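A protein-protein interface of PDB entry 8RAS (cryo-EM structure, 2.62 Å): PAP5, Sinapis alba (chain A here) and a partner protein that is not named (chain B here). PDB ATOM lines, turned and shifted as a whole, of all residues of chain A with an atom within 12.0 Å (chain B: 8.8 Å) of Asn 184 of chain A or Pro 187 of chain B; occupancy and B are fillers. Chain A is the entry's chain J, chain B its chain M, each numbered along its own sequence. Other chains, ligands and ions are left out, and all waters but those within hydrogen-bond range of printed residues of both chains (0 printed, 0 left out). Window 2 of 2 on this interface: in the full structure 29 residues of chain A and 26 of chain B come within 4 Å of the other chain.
The backbone carbonyl oxygen (O) of Val 265 of chain B is in hydrogen-bond range of the backbone NH (N) of Val 188 of chain A, 3.2 Å away.
OE1 of Glu 248 of chain B sits at hydrogen-bond distance from OH of Tyr 189 of chain A, at 3.3 Å.
The backbone NH (N) of Val 265 of chain B is in hydrogen-bond range of the backbone carbonyl oxygen (O) of Phe 186 of chain A (2.9 Å).
The backbone carbonyl oxygen (O) of Glu 248 of chain B sits at hydrogen-bond distance from the guanidinium group (NH2) of Arg 262 of chain B (3.0 Å).
N of Ala 263 of chain B lies within hydrogen-bond range of O of Ile 250 of chain B (2.8 Å).
The side-chain carboxylate (OE1) of Glu 249 of chain B lies within salt-bridge range of the guanidinium group (NH2) of Arg 262 of chain B (2.7 Å).
ND2 of Asn 184 of chain A touches CG of Pro 187 of chain B (3.7 Å).
CZ of Phe 186 of chain A touches CB of Ala 186 of chain B, 3.7 Å away.
CZ of Phe 186 of chain A touches CD of Pro 187 of chain B (3.98 Å).
Phe 186 of chain A touches Arg 262 of chain B.
Phe 186 of chain A touches Ala 263 of chain B.
Phe 186 of chain A touches Arg 264 of chain B.
CG2 of Val 187 of chain A touches O of Glu 248 of chain B, at 3.6 Å.
O of Val 265 of chain B touches CA of Val 187 of chain A, at 3.2 Å.
OH of Tyr 189 of chain A touches CG of Arg 273 of chain B, at 3.8 Å.
Asn 184 of chain A touches one residue of chain B.
Gly 185 of chain A touches none of the printed residues of chain B.
Of the printed residues of chain B, Val 187 of chain A touches Glu 248 (3.6 Å) and Val 265 (3.2 Å).
Of the printed residues of chain B, Val 188 of chain A touches Val 265 (3.2 Å).
Met 169 of chain B touches none of the printed residues of chain A.
Of chain A, only Phe 186 (3.7 Å) comes within 4 Å of Ala 186 of chain B.
Pro 187 of chain B touches two residues of chain A.
No residue of chain A comes within 4 Å of Met 188 of chain B.
No residue of chain A comes within 4 Å of Pro 189 of chain B.
Of the printed residues of chain A, Arg 264 of chain B touches Phe 186 (3.3 Å).
Of the printed residues of chain A, Val 265 of chain B touches Phe 186 (2.9 Å), Val 187 (3.2 Å) and Val 188 (3.2 Å).
Of the printed residues of chain A, Arg 273 of chain B touches Tyr 189 (3.8 Å).
The nearest residue of chain A that does not touch Pro 187 of chain B is Gly 185 of chain A (7.4 Å).
Of the 20 printed residues of chain B, 8 touch a printed residue of chain A.
Of the 6 printed residues of chain A, 5 touch a printed residue of chain B.
Printed residues of chain A that touch a printed residue of chain B: Asn 184, Phe 186, Val 187, Val 188 and Tyr 189.
Among the printed residues, 12 pairs touch across the chains.
Among the printed residues, no Asp or Glu carboxylate lies within 4 Å of a Lys or Arg side-chain nitrogen of the other chain.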
ATOM      1  N   ASN A 184      -1.053  28.458  -0.776  1.00  0.00           N
ATOM      2  CA  ASN A 184      -1.769  27.477  -1.585  1.00  0.00           C
ATOM      3  C   ASN A 184      -2.690  26.622  -0.720  1.00  0.00           C
ATOM      4  O   ASN A 184      -3.276  27.107   0.247  1.00  0.00           O
ATOM      5  CB  ASN A 184      -0.786  26.587  -2.346  1.00  0.00           C
ATOM      6  CG  ASN A 184      -0.106  27.315  -3.489  1.00  0.00           C
ATOM      7  OD1 ASN A 184      -0.754  28.012  -4.270  1.00  0.00           O
ATOM      8  ND2 ASN A 184       1.207  27.155  -3.595  1.00  0.00           N
ATOM      9  N   GLY A 185      -2.810  25.346  -1.075  1.00  0.00           N
ATOM     10  CA  GLY A 185      -3.647  24.428  -0.328  1.00  0.00           C
ATOM     11  C   GLY A 185      -2.955  23.840   0.884  1.00  0.00           C
ATOM     12  O   GLY A 185      -3.245  22.709   1.287  1.00  0.00           O
ATOM     13  N   PHE A 186      -2.035  24.602   1.477  1.00  0.00           N
ATOM     14  CA  PHE A 186      -1.311  24.160   2.660  1.00  0.00           C
ATOM     15  C   PHE A 186      -1.882  24.716   3.957  1.00  0.00           C
ATOM     16  O   PHE A 186      -1.626  24.143   5.021  1.00  0.00           O
ATOM     17  CB  PHE A 186       0.167  24.553   2.554  1.00  0.00           C
ATOM     18  CG  PHE A 186       0.905  23.844   1.457  1.00  0.00           C
ATOM     19  CD1 PHE A 186       0.911  24.350   0.168  1.00  0.00           C
ATOM     20  CD2 PHE A 186       1.604  22.677   1.714  1.00  0.00           C
ATOM     21  CE1 PHE A 186       1.590  23.702  -0.843  1.00  0.00           C
ATOM     22  CE2 PHE A 186       2.285  22.023   0.706  1.00  0.00           C
ATOM     23  CZ  PHE A 186       2.279  22.536  -0.573  1.00  0.00           C
ATOM     24  N   VAL A 187      -2.642  25.805   3.894  1.00  0.00           N
ATOM     25  CA  VAL A 187      -3.254  26.417   5.068  1.00  0.00           C
ATOM     26  C   VAL A 187      -4.761  26.257   4.946  1.00  0.00           C
ATOM     27  O   VAL A 187      -5.358  26.663   3.940  1.00  0.00           O
ATOM     28  CB  VAL A 187      -2.862  27.895   5.208  1.00  0.00           C
ATOM     29  CG1 VAL A 187      -3.266  28.422   6.575  1.00  0.00           C
ATOM     30  CG2 VAL A 187      -1.368  28.068   4.984  1.00  0.00           C
ATOM     31  N   VAL A 188      -5.376  25.665   5.967  1.00  0.00           N
ATOM     32  CA  VAL A 188      -6.811  25.403   5.992  1.00  0.00           C
ATOM     33  C   VAL A 188      -7.389  26.046   7.243  1.00  0.00           C
ATOM     34  O   VAL A 188      -6.837  25.889   8.338  1.00  0.00           O
ATOM     35  CB  VAL A 188      -7.115  23.895   5.961  1.00  0.00           C
ATOM     36  CG1 VAL A 188      -8.617  23.657   5.910  1.00  0.00           C
ATOM     37  CG2 VAL A 188      -6.426  23.235   4.776  1.00  0.00           C
ATOM     38  N   TYR A 189      -8.495  26.766   7.080  1.00  0.00           N
ATOM     39  CA  TYR A 189      -9.164  27.440   8.185  1.00  0.00           C
ATOM     40  C   TYR A 189     -10.422  26.671   8.564  1.00  0.00           C
ATOM     41  O   TYR A 189     -11.249  26.359   7.701  1.00  0.00           O
ATOM     42  CB  TYR A 189      -9.521  28.880   7.813  1.00  0.00           C
ATOM     43  CG  TYR A 189      -8.334  29.732   7.430  1.00  0.00           C
ATOM     44  CD1 TYR A 189      -7.870  29.763   6.122  1.00  0.00           C
ATOM     45  CD2 TYR A 189      -7.678  30.508   8.376  1.00  0.00           C
ATOM     46  CE1 TYR A 189      -6.786  30.541   5.767  1.00  0.00           C
ATOM     47  CE2 TYR A 189      -6.594  31.290   8.031  1.00  0.00           C
ATOM     48  CZ  TYR A 189      -6.152  31.302   6.725  1.00  0.00           C
ATOM     49  OH  TYR A 189      -5.072  32.080   6.377  1.00  0.00           O
ATOM     50  N   PHE B 166      15.688  30.477  -1.361  1.00  0.00           N
ATOM     51  CA  PHE B 166      15.378  29.073  -1.593  1.00  0.00           C
ATOM     52  C   PHE B 166      15.544  28.647  -3.045  1.00  0.00           C
ATOM     53  O   PHE B 166      15.312  27.474  -3.358  1.00  0.00           O
ATOM     54  CB  PHE B 166      13.948  28.770  -1.134  1.00  0.00           C
ATOM     55  CG  PHE B 166      13.775  28.782   0.357  1.00  0.00           C
ATOM     56  CD1 PHE B 166      13.608  29.976   1.038  1.00  0.00           C
ATOM     57  CD2 PHE B 166      13.777  27.602   1.077  1.00  0.00           C
ATOM     58  CE1 PHE B 166      13.447  29.990   2.409  1.00  0.00           C
ATOM     59  CE2 PHE B 166      13.618  27.610   2.447  1.00  0.00           C
ATOM     60  CZ  PHE B 166      13.453  28.806   3.114  1.00  0.00           C
ATOM     61  N   MET B 169      19.657  25.418  -3.709  1.00  0.00           N
ATOM     62  CA  MET B 169      19.705  24.554  -2.542  1.00  0.00           C
ATOM     63  C   MET B 169      20.559  23.335  -2.854  1.00  0.00           C
ATOM     64  O   MET B 169      20.630  22.887  -4.001  1.00  0.00           O
ATOM     65  CB  MET B 169      18.291  24.138  -2.119  1.00  0.00           C
ATOM     66  CG  MET B 169      17.706  24.990  -1.005  1.00  0.00           C
ATOM     67  SD  MET B 169      15.908  24.922  -0.916  1.00  0.00           S
ATOM     68  CE  MET B 169      15.585  23.354  -1.713  1.00  0.00           C
ATOM     69  N   VAL B 184      12.554  18.188  -3.575  1.00  0.00           N
ATOM     70  CA  VAL B 184      11.571  19.181  -3.154  1.00  0.00           C
ATOM     71  C   VAL B 184      10.182  18.579  -3.301  1.00  0.00           C
ATOM     72  O   VAL B 184       9.841  18.035  -4.359  1.00  0.00           O
ATOM     73  CB  VAL B 184      11.702  20.479  -3.967  1.00  0.00           C
ATOM     74  CG1 VAL B 184      10.939  21.593  -3.291  1.00  0.00           C
ATOM     75  CG2 VAL B 184      13.165  20.856  -4.127  1.00  0.00           C
ATOM     76  N   LEU B 185       9.382  18.675  -2.239  1.00  0.00           N
ATOM     77  CA  LEU B 185       8.043  18.101  -2.206  1.00  0.00           C
ATOM     78  C   LEU B 185       6.931  19.137  -2.280  1.00  0.00           C
ATOM     79  O   LEU B 185       5.756  18.763  -2.221  1.00  0.00           O
ATOM     80  CB  LEU B 185       7.862  17.259  -0.937  1.00  0.00           C
ATOM     81  CG  LEU B 185       7.963  15.736  -1.034  1.00  0.00           C
ATOM     82  CD1 LEU B 185       6.724  15.160  -1.697  1.00  0.00           C
ATOM     83  CD2 LEU B 185       9.206  15.328  -1.789  1.00  0.00           C
ATOM     84  N   ALA B 186       7.255  20.421  -2.410  1.00  0.00           N
ATOM     85  CA  ALA B 186       6.245  21.468  -2.367  1.00  0.00           C
ATOM     86  C   ALA B 186       6.797  22.703  -3.062  1.00  0.00           C
ATOM     87  O   ALA B 186       8.013  22.816  -3.257  1.00  0.00           O
ATOM     88  CB  ALA B 186       5.845  21.795  -0.918  1.00  0.00           C
ATOM     89  N   PRO B 187       5.932  23.632  -3.468  1.00  0.00           N
ATOM     90  CA  PRO B 187       6.423  24.900  -4.023  1.00  0.00           C
ATOM     91  C   PRO B 187       7.323  25.626  -3.036  1.00  0.00           C
ATOM     92  O   PRO B 187       7.078  25.633  -1.828  1.00  0.00           O
ATOM     93  CB  PRO B 187       5.141  25.698  -4.296  1.00  0.00           C
ATOM     94  CG  PRO B 187       3.990  24.777  -4.033  1.00  0.00           C
ATOM     95  CD  PRO B 187       4.505  23.411  -3.750  1.00  0.00           C
ATOM     96  N   MET B 188       8.376  26.244  -3.567  1.00  0.00           N
ATOM     97  CA  MET B 188       9.346  26.973  -2.770  1.00  0.00           C
ATOM     98  C   MET B 188       9.245  28.472  -3.037  1.00  0.00           C
ATOM     99  O   MET B 188       8.809  28.889  -4.114  1.00  0.00           O
ATOM    100  CB  MET B 188      10.774  26.500  -3.069  1.00  0.00           C
ATOM    101  CG  MET B 188      11.052  25.076  -2.631  1.00  0.00           C
ATOM    102  SD  MET B 188      11.245  24.925  -0.844  1.00  0.00           S
ATOM    103  CE  MET B 188       9.762  24.017  -0.417  1.00  0.00           C
ATOM    104  N   PRO B 189       9.631  29.307  -2.072  1.00  0.00           N
ATOM    105  CA  PRO B 189       9.557  30.757  -2.282  1.00  0.00           C
ATOM    106  C   PRO B 189      10.501  31.213  -3.383  1.00  0.00           C
ATOM    107  O   PRO B 189      11.559  30.621  -3.613  1.00  0.00           O
ATOM    108  CB  PRO B 189       9.970  31.340  -0.924  1.00  0.00           C
ATOM    109  CG  PRO B 189       9.889  30.214   0.036  1.00  0.00           C
ATOM    110  CD  PRO B 189      10.117  28.964  -0.727  1.00  0.00           C
ATOM    111  N   GLN B 190      10.102  32.281  -4.068  1.00  0.00           N
ATOM    112  CA  GLN B 190      10.925  32.888  -5.106  1.00  0.00           C
ATOM    113  C   GLN B 190      11.584  34.182  -4.661  1.00  0.00           C
ATOM    114  O   GLN B 190      12.640  34.541  -5.192  1.00  0.00           O
ATOM    115  CB  GLN B 190      10.086  33.151  -6.360  1.00  0.00           C
ATOM    116  CG  GLN B 190       9.285  31.948  -6.831  1.00  0.00           C
ATOM    117  CD  GLN B 190      10.164  30.772  -7.214  1.00  0.00           C
ATOM    118  OE1 GLN B 190       9.831  29.620  -6.940  1.00  0.00           O
ATOM    119  NE2 GLN B 190      11.291  31.060  -7.856  1.00  0.00           N
ATOM    120  N   GLU B 248       1.813  30.349   9.485  1.00  0.00           N
ATOM    121  CA  GLU B 248       1.244  29.800   8.262  1.00  0.00           C
ATOM    122  C   GLU B 248       2.296  29.530   7.197  1.00  0.00           C
ATOM    123  O   GLU B 248       1.967  28.952   6.156  1.00  0.00           O
ATOM    124  CB  GLU B 248       0.181  30.748   7.704  1.00  0.00           C
ATOM    125  CG  GLU B 248      -0.974  31.010   8.653  1.00  0.00           C
ATOM    126  CD  GLU B 248      -1.977  31.996   8.092  1.00  0.00           C
ATOM    127  OE1 GLU B 248      -1.869  32.340   6.897  1.00  0.00           O
ATOM    128  OE2 GLU B 248      -2.874  32.426   8.846  1.00  0.00           O
ATOM    129  N   GLU B 249       3.547  29.927   7.432  1.00  0.00           N
ATOM    130  CA  GLU B 249       4.638  29.772   6.471  1.00  0.00           C
ATOM    131  C   GLU B 249       5.779  29.039   7.171  1.00  0.00           C
ATOM    132  O   GLU B 249       6.669  29.670   7.747  1.00  0.00           O
ATOM    133  CB  GLU B 249       5.082  31.131   5.934  1.00  0.00           C
ATOM    134  CG  GLU B 249       5.743  31.084   4.567  1.00  0.00           C
ATOM    135  CD  GLU B 249       4.985  30.218   3.584  1.00  0.00           C
ATOM    136  OE1 GLU B 249       4.044  30.729   2.944  1.00  0.00           O
ATOM    137  OE2 GLU B 249       5.332  29.026   3.448  1.00  0.00           O
ATOM    138  N   ILE B 250       5.750  27.709   7.125  1.00  0.00           N
ATOM    139  CA  ILE B 250       6.765  26.870   7.749  1.00  0.00           C
ATOM    140  C   ILE B 250       7.256  25.858   6.725  1.00  0.00           C
ATOM    141  O   ILE B 250       6.446  25.205   6.057  1.00  0.00           O
ATOM    142  CB  ILE B 250       6.228  26.152   9.003  1.00  0.00           C
ATOM    143  CG1 ILE B 250       5.719  27.165  10.028  1.00  0.00           C
ATOM    144  CG2 ILE B 250       7.304  25.271   9.623  1.00  0.00           C
ATOM    145  CD1 ILE B 250       4.937  26.542  11.155  1.00  0.00           C
ATOM    146  N   TYR B 251       8.574  25.730   6.602  1.00  0.00           N
ATOM    147  CA  TYR B 251       9.200  24.776   5.696  1.00  0.00           C
ATOM    148  C   TYR B 251       9.971  23.750   6.511  1.00  0.00           C
ATOM    149  O   TYR B 251      10.750  24.114   7.398  1.00  0.00           O
ATOM    150  CB  TYR B 251      10.122  25.487   4.702  1.00  0.00           C
ATOM    151  CG  TYR B 251       9.430  26.600   3.954  1.00  0.00           C
ATOM    152  CD1 TYR B 251       8.519  26.320   2.947  1.00  0.00           C
ATOM    153  CD2 TYR B 251       9.673  27.929   4.268  1.00  0.00           C
ATOM    154  CE1 TYR B 251       7.877  27.331   2.267  1.00  0.00           C
ATOM    155  CE2 TYR B 251       9.036  28.948   3.594  1.00  0.00           C
ATOM    156  CZ  TYR B 251       8.139  28.643   2.592  1.00  0.00           C
ATOM    157  OH  TYR B 251       7.496  29.653   1.916  1.00  0.00           O
ATOM    158  N   ILE B 260      13.001  18.682   1.449  1.00  0.00           N
ATOM    159  CA  ILE B 260      12.442  19.872   2.079  1.00  0.00           C
ATOM    160  C   ILE B 260      10.994  20.011   1.626  1.00  0.00           C
ATOM    161  O   ILE B 260      10.690  19.843   0.441  1.00  0.00           O
ATOM    162  CB  ILE B 260      13.255  21.136   1.739  1.00  0.00           C
ATOM    163  CG1 ILE B 260      12.517  22.397   2.193  1.00  0.00           C
ATOM    164  CG2 ILE B 260      13.562  21.186   0.254  1.00  0.00           C
ATOM    165  CD1 ILE B 260      13.423  23.585   2.415  1.00  0.00           C
ATOM    166  N   THR B 261      10.101  20.306   2.570  1.00  0.00           N
ATOM    167  CA  THR B 261       8.673  20.378   2.297  1.00  0.00           C
ATOM    168  C   THR B 261       8.089  21.589   3.009  1.00  0.00           C
ATOM    169  O   THR B 261       8.706  22.162   3.909  1.00  0.00           O
ATOM    170  CB  THR B 261       7.953  19.098   2.749  1.00  0.00           C
ATOM    171  OG1 THR B 261       8.793  17.964   2.500  1.00  0.00           O
ATOM    172  CG2 THR B 261       6.639  18.912   2.002  1.00  0.00           C
ATOM    173  N   ARG B 262       6.888  21.980   2.591  1.00  0.00           N
ATOM    174  CA  ARG B 262       6.122  23.018   3.264  1.00  0.00           C
ATOM    175  C   ARG B 262       5.112  22.379   4.206  1.00  0.00           C
ATOM    176  O   ARG B 262       4.495  21.363   3.875  1.00  0.00           O
ATOM    177  CB  ARG B 262       5.405  23.916   2.256  1.00  0.00           C
ATOM    178  CG  ARG B 262       4.934  25.235   2.840  1.00  0.00           C
ATOM    179  CD  ARG B 262       3.637  25.684   2.198  1.00  0.00           C
ATOM    180  NE  ARG B 262       2.999  26.765   2.939  1.00  0.00           N
ATOM    181  CZ  ARG B 262       2.729  27.959   2.434  1.00  0.00           C
ATOM    182  NH1 ARG B 262       3.034  28.267   1.185  1.00  0.00           N
ATOM    183  NH2 ARG B 262       2.140  28.871   3.203  1.00  0.00           N
ATOM    184  N   ALA B 263       4.947  22.982   5.379  1.00  0.00           N
ATOM    185  CA  ALA B 263       4.104  22.410   6.418  1.00  0.00           C
ATOM    186  C   ALA B 263       2.626  22.603   6.105  1.00  0.00           C
ATOM    187  O   ALA B 263       2.208  23.661   5.626  1.00  0.00           O
ATOM    188  CB  ALA B 263       4.434  23.034   7.774  1.00  0.00           C
ATOM    189  N   ARG B 264       1.835  21.568   6.387  1.00  0.00           N
ATOM    190  CA  ARG B 264       0.380  21.618   6.251  1.00  0.00           C
ATOM    191  C   ARG B 264      -0.185  22.205   7.538  1.00  0.00           C
ATOM    192  O   ARG B 264      -0.439  21.495   8.511  1.00  0.00           O
ATOM    193  CB  ARG B 264      -0.182  20.229   5.972  1.00  0.00           C
ATOM    194  CG  ARG B 264      -1.171  20.167   4.822  1.00  0.00           C
ATOM    195  CD  ARG B 264      -0.556  20.693   3.540  1.00  0.00           C
ATOM    196  NE  ARG B 264       0.553  19.865   3.081  1.00  0.00           N
ATOM    197  CZ  ARG B 264       0.465  18.964   2.112  1.00  0.00           C
ATOM    198  NH1 ARG B 264      -0.673  18.743   1.475  1.00  0.00           N
ATOM    199  NH2 ARG B 264       1.546  18.268   1.774  1.00  0.00           N
ATOM    200  N   VAL B 265      -0.390  23.517   7.542  1.00  0.00           N
ATOM    201  CA  VAL B 265      -0.795  24.239   8.742  1.00  0.00           C
ATOM    202  C   VAL B 265      -2.314  24.339   8.784  1.00  0.00           C
ATOM    203  O   VAL B 265      -2.949  24.733   7.799  1.00  0.00           O
ATOM    204  CB  VAL B 265      -0.149  25.633   8.787  1.00  0.00           C
ATOM    205  CG1 VAL B 265      -0.723  26.446   9.930  1.00  0.00           C
ATOM    206  CG2 VAL B 265       1.357  25.509   8.920  1.00  0.00           C
ATOM    207  N   ARG B 273      -7.729  34.997   7.551  1.00  0.00           N
ATOM    208  CA  ARG B 273      -6.494  35.584   7.040  1.00  0.00           C
ATOM    209  C   ARG B 273      -6.053  36.779   7.877  1.00  0.00           C
ATOM    210  O   ARG B 273      -4.859  36.943   8.151  1.00  0.00           O
ATOM    211  CB  ARG B 273      -6.675  35.995   5.578  1.00  0.00           C
ATOM    212  CG  ARG B 273      -7.058  34.853   4.653  1.00  0.00           C
ATOM    213  CD  ARG B 273      -6.477  35.050   3.262  1.00  0.00           C
ATOM    214  NE  ARG B 273      -6.913  34.015   2.334  1.00  0.00           N
ATOM    215  CZ  ARG B 273      -6.332  33.756   1.171  1.00  0.00           C
ATOM    216  NH1 ARG B 273      -5.281  34.444   0.756  1.00  0.00           N
ATOM    217  NH2 ARG B 273      -6.817  32.784   0.404  1.00  0.00           N
